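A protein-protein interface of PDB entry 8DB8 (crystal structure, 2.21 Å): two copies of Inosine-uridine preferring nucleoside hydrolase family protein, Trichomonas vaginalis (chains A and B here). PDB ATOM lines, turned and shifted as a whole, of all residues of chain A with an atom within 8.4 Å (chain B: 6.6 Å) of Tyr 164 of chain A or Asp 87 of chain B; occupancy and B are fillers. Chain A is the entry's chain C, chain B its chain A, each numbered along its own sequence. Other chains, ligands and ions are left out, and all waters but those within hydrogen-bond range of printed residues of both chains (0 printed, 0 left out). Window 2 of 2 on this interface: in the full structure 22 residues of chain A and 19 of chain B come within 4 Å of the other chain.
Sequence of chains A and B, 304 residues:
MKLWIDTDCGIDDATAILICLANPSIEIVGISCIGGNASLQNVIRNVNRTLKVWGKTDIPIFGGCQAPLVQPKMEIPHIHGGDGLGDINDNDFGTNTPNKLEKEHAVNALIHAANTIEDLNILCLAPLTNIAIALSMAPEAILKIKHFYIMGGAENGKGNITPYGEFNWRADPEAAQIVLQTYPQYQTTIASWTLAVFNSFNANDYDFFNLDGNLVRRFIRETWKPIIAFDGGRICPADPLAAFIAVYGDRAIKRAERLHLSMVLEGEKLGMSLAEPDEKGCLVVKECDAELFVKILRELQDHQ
N of Tyr 164 of chain A lies within hydrogen-bond range of O of Ile 79 of chain B (3.1 Å).
N of Asp 87 of chain B lies within hydrogen-bond range of OD1 of Asp 83 of chain B, at 2.8 Å.
OD1 of Asp 87 of chain B is in hydrogen-bond range of N of Gly 82 of chain B (3.1 Å).
The indole nitrogen (NE1) of Trp 193 of chain A is in hydrogen-bond range of the backbone carbonyl oxygen (O) of Tyr 164 of chain A, 2.8 Å away.
Among the printed residues, pairs that only touch across the chains: Ile 161 of chain A with Pro 226 of chain B, Ile 161 of chain A with Phe 230 of chain B, Pro 163 of chain A with Ile 79 of chain B, Pro 163 of chain A with Phe 230 of chain B, Tyr 164 of chain A with His 78 of chain B, Tyr 164 of chain A with Gly 81 of chain B, Tyr 164 of chain A with Gly 82 of chain B, Tyr 164 of chain A with Asp 87 of chain B, Trp 193 of chain A with Ile 79 of chain B and Val 197 of chain A with Phe 230 of chain B.
Printed residues of chain B within 4 Å of Ile 161 of chain A: Pro 226 (3.9 Å) and Phe 230 (3.6 Å).
Of the printed residues of chain B, Trp 193 of chain A touches Ile 79.
Thr 194 of chain A touches none of the printed residues of chain B.
Of the printed residues of chain B, Val 197 of chain A touches Phe 230.
Printed residues of chain A within 4 Å of Gly 81 of chain B: Tyr 164.
No residue of chain A comes within 4 Å of Gly 86 of chain B.
Of the printed residues of chain A, Asp 87 of chain B touches Tyr 164.
The nearest printed residue of chain A that does not touch His 78 of chain B is Gly 165 of chain A (4.4 Å).
Hydrophobic or aromatic side chains of chain B within 4 Å of the printed part of chain A: Ile 79 and Phe 230.
Along chain A the printed residues that touch a printed residue of chain B span positions 161 to 197.
Among the printed residues, 11 pairs touch across the chains.
Among the printed residues, no Asp or Glu carboxylate lies within 4 Å of a Lys or Arg side-chain nitrogen of the other chain.
No position is printed for both chains.
Of the 11 pairs that touch across the chains among the printed residues, none has its exchanged pair printed and touching as well.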
ATOM      1  N   GLU A  75      19.253  11.979 -28.089  1.00  0.00           N
ATOM      2  CA  GLU A  75      18.469  12.403 -26.937  1.00  0.00           C
ATOM      3  C   GLU A  75      18.767  13.859 -26.599  1.00  0.00           C
ATOM      4  O   GLU A  75      17.919  14.568 -26.055  1.00  0.00           O
ATOM      5  CB  GLU A  75      18.760  11.511 -25.729  1.00  0.00           C
ATOM      6  CG  GLU A  75      17.885  11.799 -24.519  1.00  0.00           C
ATOM      7  CD  GLU A  75      16.613  10.972 -24.509  1.00  0.00           C
ATOM      8  OE1 GLU A  75      16.212  10.483 -25.586  1.00  0.00           O
ATOM      9  OE2 GLU A  75      16.016  10.812 -23.425  1.00  0.00           O
ATOM     10  N   ILE A  76      19.978  14.300 -26.925  1.00  0.00           N
ATOM     11  CA  ILE A  76      20.392  15.672 -26.662  1.00  0.00           C
ATOM     12  C   ILE A  76      21.058  16.305 -27.883  1.00  0.00           C
ATOM     13  O   ILE A  76      22.275  16.482 -27.907  1.00  0.00           O
ATOM     14  CB  ILE A  76      21.359  15.752 -25.464  1.00  0.00           C
ATOM     15  CG1 ILE A  76      20.657  15.315 -24.178  1.00  0.00           C
ATOM     16  CG2 ILE A  76      21.910  17.162 -25.316  1.00  0.00           C
ATOM     17  CD1 ILE A  76      21.035  13.924 -23.717  1.00  0.00           C
ATOM     18  N   ALA A 154      27.050   5.193 -16.752  1.00  0.00           N
ATOM     19  CA  ALA A 154      26.942   5.792 -15.421  1.00  0.00           C
ATOM     20  C   ALA A 154      26.593   4.674 -14.443  1.00  0.00           C
ATOM     21  O   ALA A 154      25.447   4.220 -14.396  1.00  0.00           O
ATOM     22  CB  ALA A 154      25.903   6.906 -15.390  1.00  0.00           C
ATOM     23  N   ILE A 161      24.069   6.948  -5.421  1.00  0.00           N
ATOM     24  CA  ILE A 161      23.609   8.007  -6.308  1.00  0.00           C
ATOM     25  C   ILE A 161      24.192   7.779  -7.696  1.00  0.00           C
ATOM     26  O   ILE A 161      25.342   7.347  -7.840  1.00  0.00           O
ATOM     27  CB  ILE A 161      23.990   9.400  -5.749  1.00  0.00           C
ATOM     28  CG1 ILE A 161      22.907  10.433  -6.060  1.00  0.00           C
ATOM     29  CG2 ILE A 161      25.347   9.870  -6.256  1.00  0.00           C
ATOM     30  CD1 ILE A 161      22.904  11.598  -5.097  1.00  0.00           C
ATOM     31  N   THR A 162      23.387   8.033  -8.722  1.00  0.00           N
ATOM     32  CA  THR A 162      23.827   7.934 -10.113  1.00  0.00           C
ATOM     33  C   THR A 162      23.465   9.222 -10.838  1.00  0.00           C
ATOM     34  O   THR A 162      22.263   9.519 -11.008  1.00  0.00           O
ATOM     35  CB  THR A 162      23.211   6.734 -10.827  1.00  0.00           C
ATOM     36  OG1 THR A 162      23.441   5.546 -10.057  1.00  0.00           O
ATOM     37  CG2 THR A 162      23.832   6.569 -12.208  1.00  0.00           C
ATOM     38  N   PRO A 163      24.445  10.003 -11.285  1.00  0.00           N
ATOM     39  CA  PRO A 163      24.126  11.262 -11.965  1.00  0.00           C
ATOM     40  C   PRO A 163      23.386  11.010 -13.269  1.00  0.00           C
ATOM     41  O   PRO A 163      23.714  10.097 -14.029  1.00  0.00           O
ATOM     42  CB  PRO A 163      25.502  11.900 -12.209  1.00  0.00           C
ATOM     43  CG  PRO A 163      26.470  11.116 -11.366  1.00  0.00           C
ATOM     44  CD  PRO A 163      25.891   9.751 -11.228  1.00  0.00           C
ATOM     45  N   TYR A 164      22.365  11.823 -13.507  1.00  0.00           N
ATOM     46  CA  TYR A 164      21.626  11.785 -14.756  1.00  0.00           C
ATOM     47  C   TYR A 164      22.442  12.451 -15.860  1.00  0.00           C
ATOM     48  O   TYR A 164      23.428  13.147 -15.604  1.00  0.00           O
ATOM     49  CB  TYR A 164      20.277  12.485 -14.579  1.00  0.00           C
ATOM     50  CG  TYR A 164      19.281  12.280 -15.697  1.00  0.00           C
ATOM     51  CD1 TYR A 164      18.464  11.161 -15.726  1.00  0.00           C
ATOM     52  CD2 TYR A 164      19.136  13.224 -16.706  1.00  0.00           C
ATOM     53  CE1 TYR A 164      17.544  10.976 -16.739  1.00  0.00           C
ATOM     54  CE2 TYR A 164      18.221  13.047 -17.724  1.00  0.00           C
ATOM     55  CZ  TYR A 164      17.428  11.920 -17.733  1.00  0.00           C
ATOM     56  OH  TYR A 164      16.513  11.739 -18.745  1.00  0.00           O
ATOM     57  N   GLY A 165      22.035  12.208 -17.104  1.00  0.00           N
ATOM     58  CA  GLY A 165      22.537  12.965 -18.231  1.00  0.00           C
ATOM     59  C   GLY A 165      23.585  12.286 -19.087  1.00  0.00           C
ATOM     60  O   GLY A 165      24.100  12.924 -20.014  1.00  0.00           O
ATOM     61  N   GLU A 166      23.922  11.027 -18.811  1.00  0.00           N
ATOM     62  CA  GLU A 166      24.884  10.310 -19.640  1.00  0.00           C
ATOM     63  C   GLU A 166      24.425  10.310 -21.094  1.00  0.00           C
ATOM     64  O   GLU A 166      23.258  10.031 -21.389  1.00  0.00           O
ATOM     65  CB  GLU A 166      25.051   8.879 -19.127  1.00  0.00           C
ATOM     66  CG  GLU A 166      26.265   8.145 -19.667  1.00  0.00           C
ATOM     67  CD  GLU A 166      26.005   7.514 -21.018  1.00  0.00           C
ATOM     68  OE1 GLU A 166      24.821   7.303 -21.358  1.00  0.00           O
ATOM     69  OE2 GLU A 166      26.985   7.225 -21.738  1.00  0.00           O
ATOM     70  N   PHE A 167      25.342  10.628 -22.005  1.00  0.00           N
ATOM     71  CA  PHE A 167      24.993  10.818 -23.407  1.00  0.00           C
ATOM     72  C   PHE A 167      25.433   9.678 -24.312  1.00  0.00           C
ATOM     73  O   PHE A 167      24.631   9.190 -25.115  1.00  0.00           O
ATOM     74  CB  PHE A 167      25.592  12.129 -23.933  1.00  0.00           C
ATOM     75  CG  PHE A 167      25.287  12.386 -25.385  1.00  0.00           C
ATOM     76  CD1 PHE A 167      24.084  12.956 -25.756  1.00  0.00           C
ATOM     77  CD2 PHE A 167      26.195  12.046 -26.377  1.00  0.00           C
ATOM     78  CE1 PHE A 167      23.788  13.191 -27.085  1.00  0.00           C
ATOM     79  CE2 PHE A 167      25.904  12.277 -27.711  1.00  0.00           C
ATOM     80  CZ  PHE A 167      24.700  12.852 -28.064  1.00  0.00           C
ATOM     81  N   ARG A 170      23.596   6.279 -23.937  1.00  0.00           N
ATOM     82  CA  ARG A 170      22.174   6.543 -24.112  1.00  0.00           C
ATOM     83  C   ARG A 170      21.848   6.909 -25.554  1.00  0.00           C
ATOM     84  O   ARG A 170      20.755   6.596 -26.041  1.00  0.00           O
ATOM     85  CB  ARG A 170      21.724   7.659 -23.169  1.00  0.00           C
ATOM     86  CG  ARG A 170      20.293   7.505 -22.682  1.00  0.00           C
ATOM     87  CD  ARG A 170      19.390   8.598 -23.240  1.00  0.00           C
ATOM     88  NE  ARG A 170      17.975   8.282 -23.061  1.00  0.00           N
ATOM     89  CZ  ARG A 170      17.312   7.363 -23.759  1.00  0.00           C
ATOM     90  NH1 ARG A 170      17.930   6.663 -24.703  1.00  0.00           N
ATOM     91  NH2 ARG A 170      16.025   7.149 -23.520  1.00  0.00           N
ATOM     92  N   TRP A 193      30.367   8.657 -16.908  1.00  0.00           N
ATOM     93  CA  TRP A 193      29.730   9.929 -16.591  1.00  0.00           C
ATOM     94  C   TRP A 193      29.650  10.127 -15.082  1.00  0.00           C
ATOM     95  O   TRP A 193      29.621  11.266 -14.602  1.00  0.00           O
ATOM     96  CB  TRP A 193      28.339   9.989 -17.230  1.00  0.00           C
ATOM     97  CG  TRP A 193      27.619  11.297 -17.051  1.00  0.00           C
ATOM     98  CD1 TRP A 193      26.480  11.508 -16.329  1.00  0.00           C
ATOM     99  CD2 TRP A 193      27.976  12.567 -17.616  1.00  0.00           C
ATOM    100  NE1 TRP A 193      26.112  12.828 -16.400  1.00  0.00           N
ATOM    101  CE2 TRP A 193      27.011  13.501 -17.183  1.00  0.00           C
ATOM    102  CE3 TRP A 193      29.015  13.005 -18.442  1.00  0.00           C
ATOM    103  CZ2 TRP A 193      27.055  14.848 -17.549  1.00  0.00           C
ATOM    104  CZ3 TRP A 193      29.059  14.345 -18.804  1.00  0.00           C
ATOM    105  CH2 TRP A 193      28.085  15.250 -18.356  1.00  0.00           C
ATOM    106  N   THR A 194      29.634   9.030 -14.322  1.00  0.00           N
ATOM    107  CA  THR A 194      29.696   9.130 -12.868  1.00  0.00           C
ATOM    108  C   THR A 194      31.043   9.683 -12.420  1.00  0.00           C
ATOM    109  O   THR A 194      31.111  10.567 -11.558  1.00  0.00           O
ATOM    110  CB  THR A 194      29.436   7.757 -12.244  1.00  0.00           C
ATOM    111  OG1 THR A 194      28.189   7.248 -12.729  1.00  0.00           O
ATOM    112  CG2 THR A 194      29.384   7.855 -10.725  1.00  0.00           C
ATOM    113  N   VAL A 197      31.198  13.544 -13.319  1.00  0.00           N
ATOM    114  CA  VAL A 197      30.370  14.369 -12.444  1.00  0.00           C
ATOM    115  C   VAL A 197      31.018  14.524 -11.075  1.00  0.00           C
ATOM    116  O   VAL A 197      31.038  15.621 -10.503  1.00  0.00           O
ATOM    117  CB  VAL A 197      28.952  13.773 -12.343  1.00  0.00           C
ATOM    118  CG1 VAL A 197      28.231  14.304 -11.112  1.00  0.00           C
ATOM    119  CG2 VAL A 197      28.162  14.074 -13.607  1.00  0.00           C
ATOM    120  N   CYS A 236      32.483  19.979 -16.215  1.00  0.00           N
ATOM    121  CA  CYS A 236      32.407  18.526 -16.075  1.00  0.00           C
ATOM    122  C   CYS A 236      33.224  17.895 -17.196  1.00  0.00           C
ATOM    123  O   CYS A 236      32.704  17.653 -18.295  1.00  0.00           O
ATOM    124  CB  CYS A 236      30.960  18.029 -16.110  1.00  0.00           C
ATOM    125  SG  CYS A 236      30.803  16.218 -16.084  1.00  0.00           S
ATOM    126  N   LEU A 270      15.585   2.114 -20.562  1.00  0.00           N
ATOM    127  CA  LEU A 270      16.324   2.042 -21.815  1.00  0.00           C
ATOM    128  C   LEU A 270      17.506   3.003 -21.788  1.00  0.00           C
ATOM    129  O   LEU A 270      17.365   4.175 -21.416  1.00  0.00           O
ATOM    130  CB  LEU A 270      15.397   2.369 -22.987  1.00  0.00           C
ATOM    131  CG  LEU A 270      15.957   2.309 -24.410  1.00  0.00           C
ATOM    132  CD1 LEU A 270      14.918   1.729 -25.355  1.00  0.00           C
ATOM    133  CD2 LEU A 270      16.399   3.687 -24.885  1.00  0.00           C
ATOM    134  N   MET A 272      20.360   2.580 -19.976  1.00  0.00           N
ATOM    135  CA  MET A 272      21.130   2.553 -18.745  1.00  0.00           C
ATOM    136  C   MET A 272      22.139   1.409 -18.775  1.00  0.00           C
ATOM    137  O   MET A 272      22.196   0.619 -19.720  1.00  0.00           O
ATOM    138  CB  MET A 272      20.200   2.450 -17.538  1.00  0.00           C
ATOM    139  CG  MET A 272      19.058   3.454 -17.561  1.00  0.00           C
ATOM    140  SD  MET A 272      18.653   4.089 -15.924  1.00  0.00           S
ATOM    141  CE  MET A 272      17.507   5.396 -16.356  1.00  0.00           C
ATOM    142  N   ILE B  11      15.153  22.656  -8.324  1.00  0.00           N
ATOM    143  CA  ILE B  11      15.301  22.281  -6.921  1.00  0.00           C
ATOM    144  C   ILE B  11      15.223  23.509  -6.019  1.00  0.00           C
ATOM    145  O   ILE B  11      14.421  23.557  -5.079  1.00  0.00           O
ATOM    146  CB  ILE B  11      16.612  21.507  -6.717  1.00  0.00           C
ATOM    147  CG1 ILE B  11      16.538  20.166  -7.450  1.00  0.00           C
ATOM    148  CG2 ILE B  11      16.882  21.299  -5.233  1.00  0.00           C
ATOM    149  CD1 ILE B  11      17.868  19.675  -7.958  1.00  0.00           C
ATOM    150  N   ARG B  49       4.064  19.259  -7.227  1.00  0.00           N
ATOM    151  CA  ARG B  49       4.708  18.458  -6.189  1.00  0.00           C
ATOM    152  C   ARG B  49       4.956  19.284  -4.932  1.00  0.00           C
ATOM    153  O   ARG B  49       4.674  18.837  -3.814  1.00  0.00           O
ATOM    154  CB  ARG B  49       6.025  17.883  -6.710  1.00  0.00           C
ATOM    155  CG  ARG B  49       5.880  16.799  -7.761  1.00  0.00           C
ATOM    156  CD  ARG B  49       7.220  16.537  -8.429  1.00  0.00           C
ATOM    157  NE  ARG B  49       7.428  15.127  -8.733  1.00  0.00           N
ATOM    158  CZ  ARG B  49       8.493  14.647  -9.368  1.00  0.00           C
ATOM    159  NH1 ARG B  49       9.457  15.466  -9.770  1.00  0.00           N
ATOM    160  NH2 ARG B  49       8.596  13.345  -9.599  1.00  0.00           N
ATOM    161  N   PRO B  77      22.321  19.288 -19.919  1.00  0.00           N
ATOM    162  CA  PRO B  77      22.507  17.975 -19.285  1.00  0.00           C
ATOM    163  C   PRO B  77      22.168  18.022 -17.799  1.00  0.00           C
ATOM    164  O   PRO B  77      23.001  18.398 -16.967  1.00  0.00           O
ATOM    165  CB  PRO B  77      23.990  17.680 -19.534  1.00  0.00           C
ATOM    166  CG  PRO B  77      24.628  19.042 -19.597  1.00  0.00           C
ATOM    167  CD  PRO B  77      23.596  19.994 -20.141  1.00  0.00           C
ATOM    168  N   HIS B  78      20.936  17.644 -17.460  1.00  0.00           N
ATOM    169  CA  HIS B  78      20.409  17.773 -16.099  1.00  0.00           C
ATOM    170  C   HIS B  78      21.001  16.678 -15.216  1.00  0.00           C
ATOM    171  O   HIS B  78      20.393  15.633 -14.970  1.00  0.00           O
ATOM    172  CB  HIS B  78      18.887  17.687 -16.106  1.00  0.00           C
ATOM    173  CG  HIS B  78      18.197  18.938 -16.553  1.00  0.00           C
ATOM    174  ND1 HIS B  78      18.037  19.267 -17.882  1.00  0.00           N
ATOM    175  CD2 HIS B  78      17.610  19.934 -15.845  1.00  0.00           C
ATOM    176  CE1 HIS B  78      17.386  20.413 -17.973  1.00  0.00           C
ATOM    177  NE2 HIS B  78      17.118  20.840 -16.752  1.00  0.00           N
ATOM    178  N   ILE B  79      22.209  16.930 -14.705  1.00  0.00           N
ATOM    179  CA  ILE B  79      22.890  15.931 -13.884  1.00  0.00           C
ATOM    180  C   ILE B  79      22.135  15.645 -12.593  1.00  0.00           C
ATOM    181  O   ILE B  79      22.275  14.556 -12.024  1.00  0.00           O
ATOM    182  CB  ILE B  79      24.341  16.363 -13.575  1.00  0.00           C
ATOM    183  CG1 ILE B  79      24.362  17.678 -12.790  1.00  0.00           C
ATOM    184  CG2 ILE B  79      25.149  16.471 -14.861  1.00  0.00           C
ATOM    185  CD1 ILE B  79      25.523  17.792 -11.820  1.00  0.00           C
ATOM    186  N   HIS B  80      21.331  16.594 -12.115  1.00  0.00           N
ATOM    187  CA  HIS B  80      20.564  16.395 -10.892  1.00  0.00           C
ATOM    188  C   HIS B  80      19.334  15.522 -11.095  1.00  0.00           C
ATOM    189  O   HIS B  80      18.755  15.067 -10.104  1.00  0.00           O
ATOM    190  CB  HIS B  80      20.140  17.748 -10.308  1.00  0.00           C
ATOM    191  CG  HIS B  80      21.281  18.684 -10.061  1.00  0.00           C
ATOM    192  ND1 HIS B  80      22.414  18.311  -9.369  1.00  0.00           N
ATOM    193  CD2 HIS B  80      21.467  19.977 -10.420  1.00  0.00           C
ATOM    194  CE1 HIS B  80      23.248  19.335  -9.310  1.00  0.00           C
ATOM    195  NE2 HIS B  80      22.697  20.357  -9.940  1.00  0.00           N
ATOM    196  N   GLY B  81      18.920  15.283 -12.329  1.00  0.00           N
ATOM    197  CA  GLY B  81      17.752  14.475 -12.621  1.00  0.00           C
ATOM    198  C   GLY B  81      16.996  15.023 -13.817  1.00  0.00           C
ATOM    199  O   GLY B  81      16.980  16.229 -14.085  1.00  0.00           O
ATOM    200  N   GLY B  82      16.340  14.127 -14.552  1.00  0.00           N
ATOM    201  CA  GLY B  82      15.668  14.523 -15.775  1.00  0.00           C
ATOM    202  C   GLY B  82      14.412  15.340 -15.549  1.00  0.00           C
ATOM    203  O   GLY B  82      14.057  16.179 -16.385  1.00  0.00           O
ATOM    204  N   ASP B  83      13.723  15.113 -14.428  1.00  0.00           N
ATOM    205  CA  ASP B  83      12.479  15.824 -14.155  1.00  0.00           C
ATOM    206  C   ASP B  83      12.699  17.242 -13.643  1.00  0.00           C
ATOM    207  O   ASP B  83      11.722  17.916 -13.296  1.00  0.00           O
ATOM    208  CB  ASP B  83      11.616  15.038 -13.156  1.00  0.00           C
ATOM    209  CG  ASP B  83      12.229  14.958 -11.757  1.00  0.00           C
ATOM    210  OD1 ASP B  83      13.329  15.505 -11.516  1.00  0.00           O
ATOM    211  OD2 ASP B  83      11.592  14.334 -10.882  1.00  0.00           O
ATOM    212  N   GLY B  84      13.946  17.702 -13.571  1.00  0.00           N
ATOM    213  CA  GLY B  84      14.226  19.028 -13.067  1.00  0.00           C
ATOM    214  C   GLY B  84      13.995  19.221 -11.586  1.00  0.00           C
ATOM    215  O   GLY B  84      14.079  20.356 -11.109  1.00  0.00           O
ATOM    216  N   LEU B  85      13.710  18.157 -10.840  1.00  0.00           N
ATOM    217  CA  LEU B  85      13.448  18.260  -9.406  1.00  0.00           C
ATOM    218  C   LEU B  85      14.129  17.111  -8.666  1.00  0.00           C
ATOM    219  O   LEU B  85      13.511  16.386  -7.884  1.00  0.00           O
ATOM    220  CB  LEU B  85      11.947  18.284  -9.124  1.00  0.00           C
ATOM    221  CG  LEU B  85      11.505  18.940  -7.809  1.00  0.00           C
ATOM    222  CD1 LEU B  85      11.805  20.434  -7.801  1.00  0.00           C
ATOM    223  CD2 LEU B  85      10.028  18.688  -7.554  1.00  0.00           C
ATOM    224  N   GLY B  86      15.426  16.936  -8.916  1.00  0.00           N
ATOM    225  CA  GLY B  86      16.206  15.907  -8.260  1.00  0.00           C
ATOM    226  C   GLY B  86      15.812  14.484  -8.579  1.00  0.00           C
ATOM    227  O   GLY B  86      16.351  13.560  -7.962  1.00  0.00           O
ATOM    228  N   ASP B  87      14.892  14.278  -9.524  1.00  0.00           N
ATOM    229  CA  ASP B  87      14.417  12.942  -9.893  1.00  0.00           C
ATOM    230  C   ASP B  87      13.846  12.200  -8.686  1.00  0.00           C
ATOM    231  O   ASP B  87      14.129  11.020  -8.467  1.00  0.00           O
ATOM    232  CB  ASP B  87      15.520  12.124 -10.568  1.00  0.00           C
ATOM    233  CG  ASP B  87      15.372  12.087 -12.074  1.00  0.00           C
ATOM    234  OD1 ASP B  87      14.379  12.651 -12.584  1.00  0.00           O
ATOM    235  OD2 ASP B  87      16.242  11.493 -12.746  1.00  0.00           O
ATOM    236  N   ILE B  88      13.030  12.901  -7.899  1.00  0.00           N
ATOM    237  CA  ILE B  88      12.401  12.280  -6.742  1.00  0.00           C
ATOM    238  C   ILE B  88      11.302  11.322  -7.194  1.00  0.00           C
ATOM    239  O   ILE B  88      10.779  11.402  -8.312  1.00  0.00           O
ATOM    240  CB  ILE B  88      11.847  13.346  -5.783  1.00  0.00           C
ATOM    241  CG1 ILE B  88      10.769  14.178  -6.476  1.00  0.00           C
ATOM    242  CG2 ILE B  88      12.969  14.238  -5.274  1.00  0.00           C
ATOM    243  CD1 ILE B  88      10.177  15.265  -5.596  1.00  0.00           C
ATOM    244  N   ASN B  89      10.949  10.397  -6.304  1.00  0.00           N
ATOM    245  CA  ASN B  89       9.938   9.385  -6.578  1.00  0.00           C
ATOM    246  C   ASN B  89       8.597   9.866  -6.035  1.00  0.00           C
ATOM    247  O   ASN B  89       8.456  10.087  -4.827  1.00  0.00           O
ATOM    248  CB  ASN B  89      10.332   8.045  -5.954  1.00  0.00           C
ATOM    249  CG  ASN B  89       9.474   6.891  -6.445  1.00  0.00           C
ATOM    250  OD1 ASN B  89       8.302   7.064  -6.777  1.00  0.00           O
ATOM    251  ND2 ASN B  89      10.059   5.699  -6.486  1.00  0.00           N
ATOM    252  N   GLU B 222      15.531  15.078  -0.196  1.00  0.00           N
ATOM    253  CA  GLU B 222      15.636  14.332  -1.445  1.00  0.00           C
ATOM    254  C   GLU B 222      15.854  15.238  -2.652  1.00  0.00           C
ATOM    255  O   GLU B 222      16.529  14.829  -3.603  1.00  0.00           O
ATOM    256  CB  GLU B 222      14.388  13.470  -1.647  1.00  0.00           C
ATOM    257  CG  GLU B 222      14.284  12.294  -0.675  1.00  0.00           C
ATOM    258  CD  GLU B 222      15.505  11.387  -0.709  1.00  0.00           C
ATOM    259  OE1 GLU B 222      15.930  10.994  -1.816  1.00  0.00           O
ATOM    260  OE2 GLU B 222      16.042  11.072   0.373  1.00  0.00           O
ATOM    261  N   THR B 223      15.304  16.456  -2.646  1.00  0.00           N
ATOM    262  CA  THR B 223      15.523  17.353  -3.780  1.00  0.00           C
ATOM    263  C   THR B 223      16.944  17.898  -3.784  1.00  0.00           C
ATOM    264  O   THR B 223      17.563  18.030  -4.848  1.00  0.00           O
ATOM    265  CB  THR B 223      14.511  18.505  -3.768  1.00  0.00           C
ATOM    266  OG1 THR B 223      14.499  19.137  -2.480  1.00  0.00           O
ATOM    267  CG2 THR B 223      13.114  18.003  -4.100  1.00  0.00           C
ATOM    268  N   PRO B 226      21.054  15.402  -4.735  1.00  0.00           N
ATOM    269  CA  PRO B 226      22.024  15.362  -5.840  1.00  0.00           C
ATOM    270  C   PRO B 226      22.905  16.597  -5.923  1.00  0.00           C
ATOM    271  O   PRO B 226      24.060  16.484  -6.352  1.00  0.00           O
ATOM    272  CB  PRO B 226      21.136  15.224  -7.088  1.00  0.00           C
ATOM    273  CG  PRO B 226      19.791  14.802  -6.571  1.00  0.00           C
ATOM    274  CD  PRO B 226      19.672  15.461  -5.244  1.00  0.00           C
ATOM    275  N   PHE B 230      27.048  16.035  -5.864  1.00  0.00           N
ATOM    276  CA  PHE B 230      27.871  16.250  -7.046  1.00  0.00           C
ATOM    277  C   PHE B 230      28.781  17.467  -6.950  1.00  0.00           C
ATOM    278  O   PHE B 230      29.558  17.705  -7.880  1.00  0.00           O
ATOM    279  CB  PHE B 230      26.974  16.378  -8.279  1.00  0.00           C
ATOM    280  CG  PHE B 230      26.074  15.196  -8.493  1.00  0.00           C
ATOM    281  CD1 PHE B 230      24.852  15.345  -9.128  1.00  0.00           C
ATOM    282  CD2 PHE B 230      26.452  13.931  -8.065  1.00  0.00           C
ATOM    283  CE1 PHE B 230      24.022  14.260  -9.329  1.00  0.00           C
ATOM    284  CE2 PHE B 230      25.627  12.842  -8.262  1.00  0.00           C
ATOM    285  CZ  PHE B 230      24.410  13.007  -8.895  1.00  0.00           C
